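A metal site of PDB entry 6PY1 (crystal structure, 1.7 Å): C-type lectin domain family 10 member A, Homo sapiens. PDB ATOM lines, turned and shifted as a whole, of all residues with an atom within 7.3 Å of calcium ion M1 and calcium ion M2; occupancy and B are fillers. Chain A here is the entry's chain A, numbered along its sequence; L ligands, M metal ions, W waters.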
ATOM      1  N   SER A  65     -22.829 -17.407  26.166  1.00  0.00           N
ATOM      2  CA  SER A  65     -22.728 -17.365  24.687  1.00  0.00           C
ATOM      3  C   SER A  65     -22.083 -18.647  24.179  1.00  0.00           C
ATOM      4  O   SER A  65     -21.386 -19.321  24.973  1.00  0.00           O
ATOM      5  CB  SER A  65     -21.972 -16.137  24.191  1.00  0.00           C
ATOM      6  OG  SER A  65     -20.581 -16.177  24.505  1.00  0.00           O
ATOM      7  N   ASP A  66     -22.274 -18.962  22.894  1.00  0.00           N
ATOM      8  CA  ASP A  66     -21.705 -20.226  22.348  1.00  0.00           C
ATOM      9  C   ASP A  66     -21.151 -20.065  20.940  1.00  0.00           C
ATOM     10  O   ASP A  66     -21.279 -20.999  20.159  1.00  0.00           O
ATOM     11  CB  ASP A  66     -22.730 -21.347  22.410  1.00  0.00           C
ATOM     12  CG  ASP A  66     -23.794 -21.311  21.324  1.00  0.00           C
ATOM     13  OD1 ASP A  66     -24.092 -20.195  20.825  1.00  0.00           O
ATOM     14  OD2 ASP A  66     -24.303 -22.392  20.934  1.00  0.00           O
ATOM     15  N   PRO A  67     -20.477 -18.960  20.575  1.00  0.00           N
ATOM     16  CA  PRO A  67     -20.102 -18.757  19.178  1.00  0.00           C
ATOM     17  C   PRO A  67     -19.010 -19.744  18.708  1.00  0.00           C
ATOM     18  O   PRO A  67     -18.934 -19.957  17.533  1.00  0.00           O
ATOM     19  CB  PRO A  67     -19.629 -17.306  19.133  1.00  0.00           C
ATOM     20  CG  PRO A  67     -19.087 -17.084  20.530  1.00  0.00           C
ATOM     21  CD  PRO A  67     -20.004 -17.864  21.442  1.00  0.00           C
ATOM     22  N   GLY A  69     -18.967 -23.018  19.524  1.00  0.00           N
ATOM     23  CA  GLY A  69     -19.497 -24.390  19.605  1.00  0.00           C
ATOM     24  C   GLY A  69     -20.175 -24.751  20.922  1.00  0.00           C
ATOM     25  O   GLY A  69     -21.208 -25.435  20.863  1.00  0.00           O
ATOM     26  N   TRP A  71     -21.601 -23.740  24.998  1.00  0.00           N
ATOM     27  CA  TRP A  71     -22.085 -22.643  25.905  1.00  0.00           C
ATOM     28  C   TRP A  71     -21.041 -22.356  26.965  1.00  0.00           C
ATOM     29  O   TRP A  71     -20.563 -23.308  27.634  1.00  0.00           O
ATOM     30  CB  TRP A  71     -23.452 -22.969  26.534  1.00  0.00           C
ATOM     31  CG  TRP A  71     -24.523 -22.881  25.510  1.00  0.00           C
ATOM     32  CD1 TRP A  71     -25.088 -23.871  24.786  1.00  0.00           C
ATOM     33  CD2 TRP A  71     -25.083 -21.644  25.038  1.00  0.00           C
ATOM     34  NE1 TRP A  71     -25.986 -23.349  23.904  1.00  0.00           N
ATOM     35  CE2 TRP A  71     -26.024 -21.983  24.041  1.00  0.00           C
ATOM     36  CE3 TRP A  71     -24.875 -20.296  25.356  1.00  0.00           C
ATOM     37  CZ2 TRP A  71     -26.719 -21.014  23.327  1.00  0.00           C
ATOM     38  CZ3 TRP A  71     -25.602 -19.325  24.660  1.00  0.00           C
ATOM     39  CH2 TRP A  71     -26.528 -19.697  23.672  1.00  0.00           C
ATOM     40  N   TRP A  86     -33.587 -22.454  30.772  1.00  0.00           N
ATOM     41  CA  TRP A  86     -34.017 -22.248  29.365  1.00  0.00           C
ATOM     42  C   TRP A  86     -35.537 -22.276  29.257  1.00  0.00           C
ATOM     43  O   TRP A  86     -36.212 -23.073  29.977  1.00  0.00           O
ATOM     44  CB  TRP A  86     -33.373 -23.287  28.457  1.00  0.00           C
ATOM     45  CG  TRP A  86     -31.882 -23.221  28.361  1.00  0.00           C
ATOM     46  CD1 TRP A  86     -30.983 -24.030  28.970  1.00  0.00           C
ATOM     47  CD2 TRP A  86     -31.092 -22.235  27.670  1.00  0.00           C
ATOM     48  NE1 TRP A  86     -29.715 -23.696  28.636  1.00  0.00           N
ATOM     49  CE2 TRP A  86     -29.748 -22.590  27.841  1.00  0.00           C
ATOM     50  CE3 TRP A  86     -31.401 -21.155  26.860  1.00  0.00           C
ATOM     51  CZ2 TRP A  86     -28.734 -21.853  27.284  1.00  0.00           C
ATOM     52  CZ3 TRP A  86     -30.389 -20.412  26.310  1.00  0.00           C
ATOM     53  CH2 TRP A  86     -29.071 -20.787  26.480  1.00  0.00           C
ATOM     54  N   GLY A  89     -37.996 -25.545  24.559  1.00  0.00           N
ATOM     55  CA  GLY A  89     -37.532 -25.611  23.167  1.00  0.00           C
ATOM     56  C   GLY A  89     -36.197 -24.911  22.959  1.00  0.00           C
ATOM     57  O   GLY A  89     -35.676 -25.011  21.859  1.00  0.00           O
ATOM     58  N   GLN A  90     -35.680 -24.216  23.965  1.00  0.00           N
ATOM     59  CA  GLN A  90     -34.386 -23.484  23.858  1.00  0.00           C
ATOM     60  C   GLN A  90     -33.287 -24.227  24.609  1.00  0.00           C
ATOM     61  O   GLN A  90     -33.553 -25.001  25.541  1.00  0.00           O
ATOM     62  CB  GLN A  90     -34.582 -22.066  24.404  1.00  0.00           C
ATOM     63  CG  GLN A  90     -35.723 -21.325  23.729  1.00  0.00           C
ATOM     64  CD  GLN A  90     -35.632 -21.129  22.224  1.00  0.00           C
ATOM     65  OE1 GLN A  90     -34.577 -21.146  21.639  1.00  0.00           O
ATOM     66  NE2 GLN A  90     -36.749 -20.780  21.587  1.00  0.00           N
ATOM     67  N   PRO A  91     -32.001 -24.036  24.251  1.00  0.00           N
ATOM     68  CA  PRO A  91     -31.579 -23.242  23.096  1.00  0.00           C
ATOM     69  C   PRO A  91     -31.795 -24.035  21.806  1.00  0.00           C
ATOM     70  O   PRO A  91     -31.753 -25.271  21.872  1.00  0.00           O
ATOM     71  CB  PRO A  91     -30.088 -23.044  23.327  1.00  0.00           C
ATOM     72  CG  PRO A  91     -29.655 -24.225  24.142  1.00  0.00           C
ATOM     73  CD  PRO A  91     -30.866 -24.615  24.949  1.00  0.00           C
ATOM     74  N   ASP A  92     -32.015 -23.350  20.680  1.00  0.00           N
ATOM     75  CA  ASP A  92     -32.324 -24.018  19.400  1.00  0.00           C
ATOM     76  C   ASP A  92     -31.370 -23.591  18.290  1.00  0.00           C
ATOM     77  O   ASP A  92     -31.498 -24.166  17.209  1.00  0.00           O
ATOM     78  CB  ASP A  92     -33.784 -23.819  19.011  1.00  0.00           C
ATOM     79  CG  ASP A  92     -34.193 -22.383  18.781  1.00  0.00           C
ATOM     80  OD1 ASP A  92     -33.307 -21.504  19.010  1.00  0.00           O
ATOM     81  OD2 ASP A  92     -35.379 -22.161  18.425  1.00  0.00           O
ATOM     82  N   ASP A  93     -30.438 -22.651  18.513  1.00  0.00           N
ATOM     83  CA  ASP A  93     -29.513 -22.180  17.467  1.00  0.00           C
ATOM     84  C   ASP A  93     -30.298 -21.860  16.184  1.00  0.00           C
ATOM     85  O   ASP A  93     -29.828 -22.225  15.063  1.00  0.00           O
ATOM     86  CB  ASP A  93     -28.413 -23.204  17.192  1.00  0.00           C
ATOM     87  CG  ASP A  93     -27.215 -22.623  16.437  1.00  0.00           C
ATOM     88  OD1 ASP A  93     -26.734 -21.518  16.809  1.00  0.00           O
ATOM     89  OD2 ASP A  93     -26.737 -23.298  15.496  1.00  0.00           O
ATOM     90  N   TRP A  94     -31.461 -21.244  16.332  1.00  0.00           N
ATOM     91  CA  TRP A  94     -32.385 -20.985  15.189  1.00  0.00           C
ATOM     92  C   TRP A  94     -31.666 -20.227  14.047  1.00  0.00           C
ATOM     93  O   TRP A  94     -31.001 -19.215  14.316  1.00  0.00           O
ATOM     94  CB  TRP A  94     -33.594 -20.223  15.624  1.00  0.00           C
ATOM     95  CG  TRP A  94     -34.687 -20.110  14.626  1.00  0.00           C
ATOM     96  CD1 TRP A  94     -35.329 -21.098  13.937  1.00  0.00           C
ATOM     97  CD2 TRP A  94     -35.439 -18.920  14.395  1.00  0.00           C
ATOM     98  NE1 TRP A  94     -36.377 -20.586  13.228  1.00  0.00           N
ATOM     99  CE2 TRP A  94     -36.486 -19.259  13.514  1.00  0.00           C
ATOM    100  CE3 TRP A  94     -35.347 -17.617  14.872  1.00  0.00           C
ATOM    101  CZ2 TRP A  94     -37.386 -18.302  13.046  1.00  0.00           C
ATOM    102  CZ3 TRP A  94     -36.230 -16.683  14.402  1.00  0.00           C
ATOM    103  CH2 TRP A  94     -37.254 -17.032  13.522  1.00  0.00           C
ATOM    104  N   GLY A 102     -26.767 -18.918  13.209  1.00  0.00           N
ATOM    105  CA  GLY A 102     -27.756 -19.402  14.167  1.00  0.00           C
ATOM    106  C   GLY A 102     -27.954 -18.383  15.267  1.00  0.00           C
ATOM    107  O   GLY A 102     -28.186 -17.214  14.947  1.00  0.00           O
ATOM    108  N   GLU A 103     -27.881 -18.798  16.517  1.00  0.00           N
ATOM    109  CA  GLU A 103     -28.158 -17.875  17.664  1.00  0.00           C
ATOM    110  C   GLU A 103     -27.128 -18.210  18.737  1.00  0.00           C
ATOM    111  O   GLU A 103     -27.046 -19.391  19.144  1.00  0.00           O
ATOM    112  CB  GLU A 103     -29.596 -18.014  18.176  1.00  0.00           C
ATOM    113  CG  GLU A 103     -30.687 -17.584  17.207  1.00  0.00           C
ATOM    114  CD  GLU A 103     -32.097 -17.815  17.688  1.00  0.00           C
ATOM    115  OE1 GLU A 103     -32.982 -16.890  17.543  1.00  0.00           O
ATOM    116  OE2 GLU A 103     -32.285 -18.921  18.296  1.00  0.00           O
ATOM    117  N   ASP A 104     -26.292 -17.263  19.101  1.00  0.00           N
ATOM    118  CA  ASP A 104     -25.124 -17.609  19.948  1.00  0.00           C
ATOM    119  C   ASP A 104     -25.078 -16.822  21.272  1.00  0.00           C
ATOM    120  O   ASP A 104     -24.051 -16.944  21.974  1.00  0.00           O
ATOM    121  CB  ASP A 104     -23.856 -17.412  19.120  1.00  0.00           C
ATOM    122  CG  ASP A 104     -23.750 -18.306  17.900  1.00  0.00           C
ATOM    123  OD1 ASP A 104     -24.476 -19.335  17.832  1.00  0.00           O
ATOM    124  OD2 ASP A 104     -22.975 -17.922  16.987  1.00  0.00           O
ATOM    125  N   CYS A 105     -26.090 -16.068  21.651  1.00  0.00           N
ATOM    126  CA  CYS A 105     -26.069 -15.240  22.883  1.00  0.00           C
ATOM    127  C   CYS A 105     -27.353 -15.464  23.692  1.00  0.00           C
ATOM    128  O   CYS A 105     -28.415 -15.429  23.081  1.00  0.00           O
ATOM    129  CB  CYS A 105     -25.948 -13.779  22.522  1.00  0.00           C
ATOM    130  SG  CYS A 105     -24.310 -13.341  21.893  1.00  0.00           S
ATOM    131  N   HIS A 107     -30.276 -14.559  26.510  1.00  0.00           N
ATOM    132  CA  HIS A 107     -30.981 -13.468  27.193  1.00  0.00           C
ATOM    133  C   HIS A 107     -32.117 -14.018  28.034  1.00  0.00           C
ATOM    134  O   HIS A 107     -32.673 -15.076  27.695  1.00  0.00           O
ATOM    135  CB  HIS A 107     -31.468 -12.392  26.196  1.00  0.00           C
ATOM    136  CG  HIS A 107     -32.582 -12.869  25.321  1.00  0.00           C
ATOM    137  ND1 HIS A 107     -33.892 -12.678  25.652  1.00  0.00           N
ATOM    138  CD2 HIS A 107     -32.578 -13.543  24.157  1.00  0.00           C
ATOM    139  CE1 HIS A 107     -34.671 -13.237  24.716  1.00  0.00           C
ATOM    140  NE2 HIS A 107     -33.900 -13.792  23.804  1.00  0.00           N
ATOM    141  N   TRP A 114     -34.740 -18.357  29.752  1.00  0.00           N
ATOM    142  CA  TRP A 114     -33.645 -17.956  28.847  1.00  0.00           C
ATOM    143  C   TRP A 114     -33.942 -18.409  27.413  1.00  0.00           C
ATOM    144  O   TRP A 114     -34.563 -19.479  27.170  1.00  0.00           O
ATOM    145  CB  TRP A 114     -32.298 -18.526  29.305  1.00  0.00           C
ATOM    146  CG  TRP A 114     -31.901 -18.317  30.719  1.00  0.00           C
ATOM    147  CD1 TRP A 114     -32.427 -17.501  31.650  1.00  0.00           C
ATOM    148  CD2 TRP A 114     -30.824 -19.004  31.353  1.00  0.00           C
ATOM    149  NE1 TRP A 114     -31.767 -17.624  32.833  1.00  0.00           N
ATOM    150  CE2 TRP A 114     -30.782 -18.557  32.683  1.00  0.00           C
ATOM    151  CE3 TRP A 114     -29.906 -19.956  30.917  1.00  0.00           C
ATOM    152  CZ2 TRP A 114     -29.812 -19.009  33.570  1.00  0.00           C
ATOM    153  CZ3 TRP A 114     -28.948 -20.416  31.795  1.00  0.00           C
ATOM    154  CH2 TRP A 114     -28.926 -19.956  33.107  1.00  0.00           C
ATOM    155  N   ASN A 115     -33.405 -17.627  26.487  1.00  0.00           N
ATOM    156  CA  ASN A 115     -33.459 -17.916  25.054  1.00  0.00           C
ATOM    157  C   ASN A 115     -32.085 -17.660  24.466  1.00  0.00           C
ATOM    158  O   ASN A 115     -31.446 -16.668  24.864  1.00  0.00           O
ATOM    159  CB  ASN A 115     -34.573 -17.152  24.335  1.00  0.00           C
ATOM    160  CG  ASN A 115     -34.493 -17.319  22.843  1.00  0.00           C
ATOM    161  OD1 ASN A 115     -34.516 -18.447  22.368  1.00  0.00           O
ATOM    162  ND2 ASN A 115     -34.324 -16.215  22.090  1.00  0.00           N
ATOM    163  N   ASP A 116     -31.728 -18.390  23.420  1.00  0.00           N
ATOM    164  CA  ASP A 116     -30.566 -18.033  22.576  1.00  0.00           C
ATOM    165  C   ASP A 116     -31.063 -17.162  21.409  1.00  0.00           C
ATOM    166  O   ASP A 116     -32.070 -17.471  20.753  1.00  0.00           O
ATOM    167  CB  ASP A 116     -29.744 -19.240  22.126  1.00  0.00           C
ATOM    168  CG  ASP A 116     -30.504 -20.271  21.306  1.00  0.00           C
ATOM    169  OD1 ASP A 116     -31.767 -20.354  21.420  1.00  0.00           O
ATOM    170  OD2 ASP A 116     -29.817 -20.953  20.542  1.00  0.00           O
ATOM    171  N   ASP A 117     -30.336 -16.096  21.139  1.00  0.00           N
ATOM    172  CA  ASP A 117     -30.779 -15.150  20.083  1.00  0.00           C
ATOM    173  C   ASP A 117     -29.557 -14.635  19.355  1.00  0.00           C
ATOM    174  O   ASP A 117     -28.412 -14.959  19.716  1.00  0.00           O
ATOM    175  CB  ASP A 117     -31.657 -14.024  20.700  1.00  0.00           C
ATOM    176  CG  ASP A 117     -32.760 -13.465  19.771  1.00  0.00           C
ATOM    177  OD1 ASP A 117     -32.522 -13.412  18.546  1.00  0.00           O
ATOM    178  OD2 ASP A 117     -33.901 -13.152  20.269  1.00  0.00           O
ATOM    179  N   VAL A 118     -29.840 -13.830  18.366  1.00  0.00           N
ATOM    180  CA  VAL A 118     -28.807 -13.215  17.505  1.00  0.00           C
ATOM    181  C   VAL A 118     -28.079 -12.156  18.332  1.00  0.00           C
ATOM    182  O   VAL A 118     -28.699 -11.208  18.834  1.00  0.00           O
ATOM    183  CB  VAL A 118     -29.471 -12.639  16.258  1.00  0.00           C
ATOM    184  CG1 VAL A 118     -28.481 -11.796  15.474  1.00  0.00           C
ATOM    185  CG2 VAL A 118     -30.081 -13.759  15.407  1.00  0.00           C
HETATM  186  O1  LIG L   1     -38.533 -18.810  18.634  1.00  0.00           O
HETATM  187  C1  LIG L   1     -38.455 -17.479  19.180  1.00  0.00           C
HETATM  188  O2  LIG L   1     -38.760 -16.446  18.201  1.00  0.00           O
HETATM  189  C2  LIG L   1     -37.064 -17.171  19.778  1.00  0.00           C
HETATM  190  N1  LIG L   1     -37.080 -15.768  20.199  1.00  0.00           N
HETATM  191  C3  LIG L   1     -35.943 -17.416  18.792  1.00  0.00           C
HETATM  192  O3  LIG L   1     -34.656 -17.380  19.390  1.00  0.00           O
HETATM  193  C4  LIG L   1     -36.113 -18.764  18.153  1.00  0.00           C
HETATM  194  O4  LIG L   1     -35.707 -19.680  19.156  1.00  0.00           O
HETATM  195  C5  LIG L   1     -37.548 -18.948  17.577  1.00  0.00           C
HETATM  196  C6  LIG L   1     -37.728 -20.310  16.921  1.00  0.00           C
HETATM  197  O5  LIG L   1     -39.070 -20.410  16.387  1.00  0.00           O
HETATM  198  C7  LIG L   1     -37.296 -15.431  21.501  1.00  0.00           C
HETATM  199  O6  LIG L   1     -37.526 -16.281  22.388  1.00  0.00           O
HETATM  200  C8  LIG L   1     -37.154 -13.966  21.843  1.00  0.00           C
HETATM  201 CA    CA M   1     -25.527 -21.183  18.912  1.00  0.00          CA
HETATM  202 CA    CA M   2     -33.604 -19.370  20.281  1.00  0.00          CA
HETATM  203  O   HOH W   1     -25.356 -23.659  18.437  1.00  0.00           O
HETATM  204  O   HOH W   2     -23.203 -21.924  17.984  1.00  0.00           O
HETATM  205  O   HOH W   3     -27.342 -22.064  20.137  1.00  0.00           O
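The side-chain carboxylate (OD1) of Asp 92 lies close to the backbone NH (N) of Trp 94, 3.3 Å away.
The backbone NH (N) of Trp 94 lies close to the side-chain carboxylate (OE2) of Glu 103 (3.2 Å).
The side-chain carboxylate (OD2) of Asp 116 lies within hydrogen-bond range of the backbone NH (N) of Asp 93, 2.7 Å away.
N of Asn 115 lies within hydrogen-bond range of O of His 107 (2.9 Å).
N of Asp 104 is in hydrogen-bond range of O of Asp 117 (3.2 Å).
Four residues have an atom within 4 Å of calcium ion M1: Asp 66, Asp 93, Glu 103 and Asp 104.
Five residues have an atom within 4 Å of calcium ion M2: Gln 90, Asp 92, Glu 103, Asn 115 and Asp 116.
Along chain A the residues within 4 Å of calcium ion M2 span positions 90 to 116.
Calcium ion M1 is bound by the backbone carbonyl oxygen (O) of Glu 103 (2.4 Å), water W3 (2.4 Å), the side-chain carboxylate (OD1) of Asp 104 (2.4 Å), the side-chain carboxylate (OD1) of Asp 93 (2.4 Å), water W1 (2.5 Å), the side-chain carboxylate (OD1) of Asp 66 (2.6 Å), water W2 (2.6 Å) and the side-chain carboxylate (OD2) of Asp 66 (2.7 Å).
Calcium ion M1 has eight donor atoms within binding distance.
The side-chain carboxylate (OD1) of Asp 116 binds calcium ion M2, at 2.4 Å.
An oxygen (O4) of the ligand is bound to calcium ion M2 (2.4 Å).
Calcium ion M2 is bound by an oxygen (O3) of the ligand (2.4 Å).
OE2 of Glu 103 is bound to calcium ion M2 (2.4 Å).
The side-chain amide oxygen (OE1) of Gln 90 binds calcium ion M2, 2.4 Å away.
OD1 of Asn 115 is bound to calcium ion M2, at 2.5 Å.
O of Asp 116 is bound to calcium ion M2.
OD1 of Asp 92 binds calcium ion M2 (2.5 Å).
Calcium ion M2 has eight donor atoms within binding distance.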
